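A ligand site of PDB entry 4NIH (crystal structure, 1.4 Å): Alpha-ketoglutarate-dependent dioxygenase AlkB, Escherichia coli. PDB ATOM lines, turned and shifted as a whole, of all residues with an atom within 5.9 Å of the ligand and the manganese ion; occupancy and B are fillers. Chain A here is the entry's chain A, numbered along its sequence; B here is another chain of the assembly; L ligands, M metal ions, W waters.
The backbone NH (N) of Tyr 111 is in hydrogen-bond range of the backbone carbonyl oxygen (O) of Arg 193.
N of Ile 178 is in hydrogen-bond range of O of Leu 117, at 2.9 Å.
OG1 of Thr 197 sits at hydrogen-bond distance from OD1 of Asn 195, 3.1 Å away.
OD1 of Asn 195 sits at hydrogen-bond distance from OG of Ser 134 (3.0 Å).
ND2 of Asn 109 lies close to SD of Met 50 (3.8 Å).
The guanidinium group of Arg 193 sits at hydrogen-bond distance from the side-chain hydroxyl of Ser 136 (2.9 Å).
A ring nitrogen (ND1) of His 120 is in hydrogen-bond range of O4' of 6MA 8 of chain B, 3.4 Å away.
NH2 of Arg 193 sits close to ND2 of Asn 195 (3.2 Å).
An oxygen (O1) of the ligand sits close to N1 of 6MA 8 of chain B (3.4 Å).
CD2 of Leu 107 touches O2 of the ligand (3.5 Å).
Leu 117 touches the ligand (CD2 to C2, 3.5 Å).
Ser 134 touches the ligand (OG to O4, 3.98 Å).
CD1 of Ile 178 touches O4 of the ligand, at 3.4 Å.
OG1 of Thr 197 touches O2 of the ligand (3.7 Å).
Hydrophobic or aromatic side chains that line the ligand: Leu 107, Tyr 111, Leu 117, His 120, His 176 and Ile 178.
Of the 21 residues printed, 13 come within 4 Å of the ligand.
Water W2 lies within hydrogen-bond range of N1 of 6MA 8 of chain B (2.8 Å) and the side-chain carboxylate (OD2) of Asp 122 (2.8 Å).
Water W4 bridges OG of Ser 134 (2.7 Å) and O4 of the ligand (2.7 Å).
Water W1 lies within hydrogen-bond range of the side-chain hydroxyl (OG1) of Thr 197 (2.7 Å) and the side-chain hydroxyl (OG) of Ser 134 (2.8 Å).
An oxygen (O2) of the ligand lies close to the side-chain amide oxygen of Asn 109 (2.8 Å).
The side-chain amide nitrogen of Asn 195 sits at hydrogen-bond distance from an oxygen (O4) of the ligand, 3.3 Å away.
O5 of the ligand is in hydrogen-bond range of OH of Tyr 111 (2.6 Å).
The guanidinium group (NH1) of Arg 193 is in salt-bridge range of an oxygen (O5) of the ligand (2.8 Å).
Three residues have an atom within 4 Å of the manganese ion: His 120, Asp 122 and His 176.
The nearest printed residue that does not touch the manganese ion is 6MA 8 of chain B (4.3 Å).
OD1 of Asp 122 is bound to the manganese ion, 2.1 Å away.
The manganese ion is bound by an oxygen (O1) of the ligand.
NE2 of His 176 binds the manganese ion (2.2 Å).
NE2 of His 120 binds the manganese ion (2.3 Å).
An oxygen (O3) of the ligand is bound to the manganese ion.
The manganese ion is bound by water W3 (2.3 Å).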
ATOM      1  N   MET A  50     -16.118 -22.869 -18.625  1.00  0.00           N
ATOM      2  CA  MET A  50     -16.448 -23.010 -20.038  1.00  0.00           C
ATOM      3  C   MET A  50     -15.262 -22.915 -20.965  1.00  0.00           C
ATOM      4  O   MET A  50     -14.252 -22.272 -20.661  1.00  0.00           O
ATOM      5  CB  MET A  50     -17.426 -21.903 -20.407  1.00  0.00           C
ATOM      6  CG  MET A  50     -18.814 -22.065 -19.789  1.00  0.00           C
ATOM      7  SD  MET A  50     -19.919 -20.657 -20.024  1.00  0.00           S
ATOM      8  CE  MET A  50     -21.561 -21.324 -19.717  1.00  0.00           C
ATOM      9  N   LEU A 107     -20.245 -24.841 -27.273  1.00  0.00           N
ATOM     10  CA  LEU A 107     -19.920 -24.391 -25.942  1.00  0.00           C
ATOM     11  C   LEU A 107     -19.772 -25.611 -25.042  1.00  0.00           C
ATOM     12  O   LEU A 107     -20.703 -26.416 -24.979  1.00  0.00           O
ATOM     13  CB  LEU A 107     -21.000 -23.452 -25.411  1.00  0.00           C
ATOM     14  CG  LEU A 107     -20.944 -23.036 -23.940  1.00  0.00           C
ATOM     15  CD1 LEU A 107     -19.673 -22.274 -23.647  1.00  0.00           C
ATOM     16  CD2 LEU A 107     -22.186 -22.216 -23.619  1.00  0.00           C
ATOM     17  N   ASN A 109     -19.175 -26.997 -21.347  1.00  0.00           N
ATOM     18  CA  ASN A 109     -19.362 -26.656 -19.948  1.00  0.00           C
ATOM     19  C   ASN A 109     -18.766 -27.738 -19.065  1.00  0.00           C
ATOM     20  O   ASN A 109     -18.862 -28.920 -19.401  1.00  0.00           O
ATOM     21  CB  ASN A 109     -20.871 -26.539 -19.661  1.00  0.00           C
ATOM     22  CG  ASN A 109     -21.531 -25.410 -20.445  1.00  0.00           C
ATOM     23  OD1 ASN A 109     -22.517 -25.606 -21.158  1.00  0.00           O
ATOM     24  ND2 ASN A 109     -20.976 -24.257 -20.336  1.00  0.00           N
ATOM     25  N   TYR A 111     -18.930 -28.807 -15.019  1.00  0.00           N
ATOM     26  CA  TYR A 111     -19.542 -28.622 -13.711  1.00  0.00           C
ATOM     27  C   TYR A 111     -18.793 -29.421 -12.658  1.00  0.00           C
ATOM     28  O   TYR A 111     -18.738 -30.660 -12.725  1.00  0.00           O
ATOM     29  CB  TYR A 111     -21.001 -29.117 -13.728  1.00  0.00           C
ATOM     30  CG  TYR A 111     -21.915 -28.416 -14.693  1.00  0.00           C
ATOM     31  CD1 TYR A 111     -21.897 -28.703 -16.049  1.00  0.00           C
ATOM     32  CD2 TYR A 111     -22.829 -27.470 -14.226  1.00  0.00           C
ATOM     33  CE1 TYR A 111     -22.756 -28.044 -16.921  1.00  0.00           C
ATOM     34  CE2 TYR A 111     -23.695 -26.804 -15.100  1.00  0.00           C
ATOM     35  CZ  TYR A 111     -23.640 -27.104 -16.432  1.00  0.00           C
ATOM     36  OH  TYR A 111     -24.484 -26.442 -17.297  1.00  0.00           O
ATOM     37  N   LEU A 117     -26.273 -23.611 -13.408  1.00  0.00           N
ATOM     38  CA  LEU A 117     -26.541 -22.626 -14.474  1.00  0.00           C
ATOM     39  C   LEU A 117     -27.962 -22.152 -14.308  1.00  0.00           C
ATOM     40  O   LEU A 117     -28.920 -22.876 -14.578  1.00  0.00           O
ATOM     41  CB  LEU A 117     -26.301 -23.252 -15.847  1.00  0.00           C
ATOM     42  CG  LEU A 117     -26.040 -22.321 -17.000  1.00  0.00           C
ATOM     43  CD1 LEU A 117     -24.881 -21.382 -16.713  1.00  0.00           C
ATOM     44  CD2 LEU A 117     -25.809 -23.134 -18.273  1.00  0.00           C
ATOM     45  N   HIS A 120     -32.154 -19.557 -17.953  1.00  0.00           N
ATOM     46  CA  HIS A 120     -31.873 -18.570 -18.967  1.00  0.00           C
ATOM     47  C   HIS A 120     -32.478 -19.055 -20.283  1.00  0.00           C
ATOM     48  O   HIS A 120     -32.940 -20.194 -20.402  1.00  0.00           O
ATOM     49  CB  HIS A 120     -30.350 -18.395 -19.124  1.00  0.00           C
ATOM     50  CG  HIS A 120     -29.665 -19.624 -19.601  1.00  0.00           C
ATOM     51  ND1 HIS A 120     -29.303 -20.645 -18.760  1.00  0.00           N
ATOM     52  CD2 HIS A 120     -29.280 -20.002 -20.841  1.00  0.00           C
ATOM     53  CE1 HIS A 120     -28.714 -21.606 -19.465  1.00  0.00           C
ATOM     54  NE2 HIS A 120     -28.700 -21.242 -20.728  1.00  0.00           N
ATOM     55  N   GLN A 121     -32.462 -18.170 -21.272  1.00  0.00           N
ATOM     56  CA  GLN A 121     -32.841 -18.486 -22.643  1.00  0.00           C
ATOM     57  C   GLN A 121     -31.579 -18.429 -23.483  1.00  0.00           C
ATOM     58  O   GLN A 121     -30.714 -17.582 -23.262  1.00  0.00           O
ATOM     59  CB  GLN A 121     -33.849 -17.463 -23.158  1.00  0.00           C
ATOM     60  CG  GLN A 121     -35.142 -17.353 -22.366  1.00  0.00           C
ATOM     61  CD  GLN A 121     -36.000 -16.196 -22.872  1.00  0.00           C
ATOM     62  OE1 GLN A 121     -35.749 -15.037 -22.537  1.00  0.00           O
ATOM     63  NE2 GLN A 121     -36.972 -16.496 -23.704  1.00  0.00           N
ATOM     64  N   ASP A 122     -31.468 -19.331 -24.452  1.00  0.00           N
ATOM     65  CA  ASP A 122     -30.502 -19.191 -25.540  1.00  0.00           C
ATOM     66  C   ASP A 122     -31.230 -18.368 -26.620  1.00  0.00           C
ATOM     67  O   ASP A 122     -32.052 -18.895 -27.368  1.00  0.00           O
ATOM     68  CB  ASP A 122     -30.059 -20.553 -26.093  1.00  0.00           C
ATOM     69  CG  ASP A 122     -29.027 -21.286 -25.209  1.00  0.00           C
ATOM     70  OD1 ASP A 122     -29.102 -21.250 -23.953  1.00  0.00           O
ATOM     71  OD2 ASP A 122     -28.126 -21.938 -25.817  1.00  0.00           O
ATOM     72  N   ILE A 132     -30.852 -26.316 -30.920  1.00  0.00           N
ATOM     73  CA  ILE A 132     -29.811 -26.546 -29.947  1.00  0.00           C
ATOM     74  C   ILE A 132     -29.701 -28.048 -29.704  1.00  0.00           C
ATOM     75  O   ILE A 132     -30.706 -28.697 -29.459  1.00  0.00           O
ATOM     76  CB  ILE A 132     -30.113 -25.854 -28.622  1.00  0.00           C
ATOM     77  CG1 ILE A 132     -30.129 -24.324 -28.804  1.00  0.00           C
ATOM     78  CG2 ILE A 132     -29.086 -26.247 -27.551  1.00  0.00           C
ATOM     79  CD1 ILE A 132     -30.911 -23.591 -27.745  1.00  0.00           C
ATOM     80  N   SER A 134     -27.682 -30.636 -27.126  1.00  0.00           N
ATOM     81  CA  SER A 134     -27.074 -30.467 -25.817  1.00  0.00           C
ATOM     82  C   SER A 134     -26.727 -31.841 -25.267  1.00  0.00           C
ATOM     83  O   SER A 134     -27.612 -32.632 -24.978  1.00  0.00           O
ATOM     84  CB  SER A 134     -28.057 -29.734 -24.897  1.00  0.00           C
ATOM     85  OG  SER A 134     -27.463 -29.336 -23.671  1.00  0.00           O
ATOM     86  N   SER A 136     -24.841 -34.495 -22.600  1.00  0.00           N
ATOM     87  CA  SER A 136     -24.395 -34.669 -21.212  1.00  0.00           C
ATOM     88  C   SER A 136     -23.353 -35.772 -21.116  1.00  0.00           C
ATOM     89  O   SER A 136     -23.502 -36.849 -21.726  1.00  0.00           O
ATOM     90  CB  SER A 136     -25.561 -35.102 -20.315  1.00  0.00           C
ATOM     91  OG  SER A 136     -26.566 -34.118 -20.207  1.00  0.00           O
ATOM     92  N   PHE A 143     -31.752 -31.022 -14.872  1.00  0.00           N
ATOM     93  CA  PHE A 143     -32.012 -30.051 -15.920  1.00  0.00           C
ATOM     94  C   PHE A 143     -33.426 -29.509 -15.745  1.00  0.00           C
ATOM     95  O   PHE A 143     -34.365 -30.284 -15.582  1.00  0.00           O
ATOM     96  CB  PHE A 143     -31.864 -30.757 -17.271  1.00  0.00           C
ATOM     97  CG  PHE A 143     -32.081 -29.885 -18.501  1.00  0.00           C
ATOM     98  CD1 PHE A 143     -31.216 -28.869 -18.790  1.00  0.00           C
ATOM     99  CD2 PHE A 143     -33.109 -30.164 -19.404  1.00  0.00           C
ATOM    100  CE1 PHE A 143     -31.398 -28.101 -19.926  1.00  0.00           C
ATOM    101  CE2 PHE A 143     -33.273 -29.413 -20.556  1.00  0.00           C
ATOM    102  CZ  PHE A 143     -32.416 -28.377 -20.809  1.00  0.00           C
ATOM    103  N   LEU A 159     -30.442 -35.663 -16.158  1.00  0.00           N
ATOM    104  CA  LEU A 159     -29.649 -35.955 -17.335  1.00  0.00           C
ATOM    105  C   LEU A 159     -28.422 -36.769 -16.906  1.00  0.00           C
ATOM    106  O   LEU A 159     -27.648 -36.346 -16.040  1.00  0.00           O
ATOM    107  CB  LEU A 159     -29.229 -34.676 -18.045  1.00  0.00           C
ATOM    108  CG  LEU A 159     -30.345 -33.754 -18.548  1.00  0.00           C
ATOM    109  CD1 LEU A 159     -29.736 -32.589 -19.320  1.00  0.00           C
ATOM    110  CD2 LEU A 159     -31.394 -34.460 -19.383  1.00  0.00           C
ATOM    111  N   TRP A 167     -33.664 -28.972 -28.709  1.00  0.00           N
ATOM    112  CA  TRP A 167     -34.832 -28.094 -28.771  1.00  0.00           C
ATOM    113  C   TRP A 167     -34.676 -27.067 -29.856  1.00  0.00           C
ATOM    114  O   TRP A 167     -33.571 -26.771 -30.307  1.00  0.00           O
ATOM    115  CB  TRP A 167     -35.226 -27.503 -27.402  1.00  0.00           C
ATOM    116  CG  TRP A 167     -34.282 -26.575 -26.701  1.00  0.00           C
ATOM    117  CD1 TRP A 167     -34.412 -25.216 -26.581  1.00  0.00           C
ATOM    118  CD2 TRP A 167     -33.142 -26.929 -25.895  1.00  0.00           C
ATOM    119  NE1 TRP A 167     -33.396 -24.709 -25.808  1.00  0.00           N
ATOM    120  CE2 TRP A 167     -32.611 -25.740 -25.357  1.00  0.00           C
ATOM    121  CE3 TRP A 167     -32.525 -28.146 -25.582  1.00  0.00           C
ATOM    122  CZ2 TRP A 167     -31.483 -25.738 -24.530  1.00  0.00           C
ATOM    123  CZ3 TRP A 167     -31.403 -28.132 -24.749  1.00  0.00           C
ATOM    124  CH2 TRP A 167     -30.901 -26.937 -24.233  1.00  0.00           C
ATOM    125  N   HIS A 176     -34.353 -22.561 -19.460  1.00  0.00           N
ATOM    126  CA  HIS A 176     -33.805 -23.834 -19.004  1.00  0.00           C
ATOM    127  C   HIS A 176     -32.583 -23.560 -18.153  1.00  0.00           C
ATOM    128  O   HIS A 176     -32.037 -22.456 -18.153  1.00  0.00           O
ATOM    129  CB  HIS A 176     -33.430 -24.701 -20.215  1.00  0.00           C
ATOM    130  CG  HIS A 176     -32.433 -24.040 -21.102  1.00  0.00           C
ATOM    131  ND1 HIS A 176     -32.786 -23.077 -22.006  1.00  0.00           N
ATOM    132  CD2 HIS A 176     -31.076 -24.128 -21.152  1.00  0.00           C
ATOM    133  CE1 HIS A 176     -31.708 -22.614 -22.597  1.00  0.00           C
ATOM    134  NE2 HIS A 176     -30.661 -23.230 -22.096  1.00  0.00           N
ATOM    135  N   GLY A 177     -32.159 -24.574 -17.415  1.00  0.00           N
ATOM    136  CA  GLY A 177     -30.978 -24.454 -16.602  1.00  0.00           C
ATOM    137  C   GLY A 177     -30.586 -25.733 -15.914  1.00  0.00           C
ATOM    138  O   GLY A 177     -31.168 -26.782 -16.176  1.00  0.00           O
ATOM    139  N   ILE A 178     -29.583 -25.664 -15.046  1.00  0.00           N
ATOM    140  CA  ILE A 178     -29.038 -26.813 -14.325  1.00  0.00           C
ATOM    141  C   ILE A 178     -28.960 -26.484 -12.835  1.00  0.00           C
ATOM    142  O   ILE A 178     -28.424 -25.459 -12.440  1.00  0.00           O
ATOM    143  CB  ILE A 178     -27.632 -27.196 -14.867  1.00  0.00           C
ATOM    144  CG1 ILE A 178     -27.719 -27.750 -16.283  1.00  0.00           C
ATOM    145  CG2 ILE A 178     -26.909 -28.185 -13.949  1.00  0.00           C
ATOM    146  CD1 ILE A 178     -28.211 -29.170 -16.422  1.00  0.00           C
ATOM    147  N   ARG A 193     -19.138 -33.154 -14.401  1.00  0.00           N
ATOM    148  CA  ARG A 193     -20.041 -33.300 -15.540  1.00  0.00           C
ATOM    149  C   ARG A 193     -19.578 -32.348 -16.622  1.00  0.00           C
ATOM    150  O   ARG A 193     -19.191 -31.217 -16.327  1.00  0.00           O
ATOM    151  CB  ARG A 193     -21.489 -32.969 -15.147  1.00  0.00           C
ATOM    152  CG  ARG A 193     -22.457 -32.957 -16.313  1.00  0.00           C
ATOM    153  CD  ARG A 193     -23.872 -32.644 -15.859  1.00  0.00           C
ATOM    154  NE  ARG A 193     -24.831 -32.671 -16.961  1.00  0.00           N
ATOM    155  CZ  ARG A 193     -25.251 -31.605 -17.647  1.00  0.00           C
ATOM    156  NH1 ARG A 193     -24.853 -30.379 -17.324  1.00  0.00           N
ATOM    157  NH2 ARG A 193     -26.099 -31.774 -18.645  1.00  0.00           N
ATOM    158  N   ASN A 195     -20.938 -30.754 -20.444  1.00  0.00           N
ATOM    159  CA  ASN A 195     -22.029 -30.601 -21.414  1.00  0.00           C
ATOM    160  C   ASN A 195     -21.456 -29.989 -22.688  1.00  0.00           C
ATOM    161  O   ASN A 195     -20.544 -29.165 -22.611  1.00  0.00           O
ATOM    162  CB  ASN A 195     -23.190 -29.753 -20.881  1.00  0.00           C
ATOM    163  CG  ASN A 195     -24.438 -29.866 -21.733  1.00  0.00           C
ATOM    164  OD1 ASN A 195     -24.750 -28.964 -22.520  1.00  0.00           O
ATOM    165  ND2 ASN A 195     -25.131 -30.980 -21.613  1.00  0.00           N
ATOM    166  N   THR A 197     -22.864 -27.955 -26.016  1.00  0.00           N
ATOM    167  CA  THR A 197     -24.008 -27.201 -26.552  1.00  0.00           C
ATOM    168  C   THR A 197     -23.682 -26.732 -27.952  1.00  0.00           C
ATOM    169  O   THR A 197     -22.853 -25.837 -28.126  1.00  0.00           O
ATOM    170  CB  THR A 197     -24.359 -26.006 -25.641  1.00  0.00           C
ATOM    171  OG1 THR A 197     -24.770 -26.502 -24.361  1.00  0.00           O
ATOM    172  CG2 THR A 197     -25.468 -25.138 -26.230  1.00  0.00           C
ATOM    173  P   6MA B   8     -29.403 -14.615 -17.544  1.00  0.00           P
ATOM    174  OP1 6MA B   8     -30.647 -15.397 -17.843  1.00  0.00           O
ATOM    175  OP2 6MA B   8     -28.744 -13.879 -18.669  1.00  0.00           O
ATOM    176  O5' 6MA B   8     -28.267 -15.534 -16.853  1.00  0.00           O
ATOM    177  C5' 6MA B   8     -28.545 -16.649 -16.034  1.00  0.00           C
ATOM    178  C4' 6MA B   8     -27.387 -17.624 -16.125  1.00  0.00           C
ATOM    179  O4' 6MA B   8     -27.352 -18.198 -17.448  1.00  0.00           O
ATOM    180  C3' 6MA B   8     -26.030 -16.974 -15.854  1.00  0.00           C
ATOM    181  O3' 6MA B   8     -25.047 -17.830 -15.252  1.00  0.00           O
ATOM    182  C2' 6MA B   8     -25.516 -16.735 -17.278  1.00  0.00           C
ATOM    183  C1' 6MA B   8     -26.099 -17.905 -18.056  1.00  0.00           C
ATOM    184  N9  6MA B   8     -26.412 -17.655 -19.471  1.00  0.00           N
ATOM    185  C8  6MA B   8     -27.212 -16.665 -19.955  1.00  0.00           C
ATOM    186  N7  6MA B   8     -27.358 -16.780 -21.274  1.00  0.00           N
ATOM    187  C5  6MA B   8     -26.658 -17.843 -21.692  1.00  0.00           C
ATOM    188  C6  6MA B   8     -26.397 -18.488 -22.979  1.00  0.00           C
ATOM    189  N1  6MA B   8     -25.618 -19.594 -22.943  1.00  0.00           N
ATOM    190  C2  6MA B   8     -25.093 -20.085 -21.799  1.00  0.00           C
ATOM    191  N3  6MA B   8     -25.266 -19.545 -20.597  1.00  0.00           N
ATOM    192  C4  6MA B   8     -26.052 -18.438 -20.496  1.00  0.00           C
ATOM    193  N6  6MA B   8     -26.906 -17.981 -24.121  1.00  0.00           N
ATOM    194  C1  6MA B   8     -26.573 -18.533 -25.422  1.00  0.00           C
HETATM  195  C1  LIG L   1     -25.864 -23.771 -21.884  1.00  0.00           C
HETATM  196  O1  LIG L   1     -26.437 -22.826 -22.539  1.00  0.00           O
HETATM  197  O2  LIG L   1     -24.611 -23.907 -21.790  1.00  0.00           O
HETATM  198  C2  LIG L   1     -26.746 -24.725 -21.192  1.00  0.00           C
HETATM  199  O3  LIG L   1     -27.958 -24.415 -21.121  1.00  0.00           O
HETATM  200  C3  LIG L   1     -26.153 -25.982 -20.581  1.00  0.00           C
HETATM  201  C4  LIG L   1     -27.179 -27.042 -20.222  1.00  0.00           C
HETATM  202  C5  LIG L   1     -26.560 -28.282 -19.590  1.00  0.00           C
HETATM  203  O4  LIG L   1     -27.199 -29.343 -19.700  1.00  0.00           O
HETATM  204  O5  LIG L   1     -25.436 -28.194 -19.024  1.00  0.00           O
HETATM  205 MN    MN M   1     -28.585 -22.661 -22.475  1.00  0.00          MN
HETATM  206  O   HOH W   1     -27.381 -26.502 -23.695  1.00  0.00           O
HETATM  207  O   HOH W   2     -25.538 -21.696 -24.772  1.00  0.00           O
HETATM  208  O   HOH W   3     -28.571 -24.201 -24.247  1.00  0.00           O
HETATM  209  O   HOH W   4     -28.987 -30.073 -21.581  1.00  0.00           O
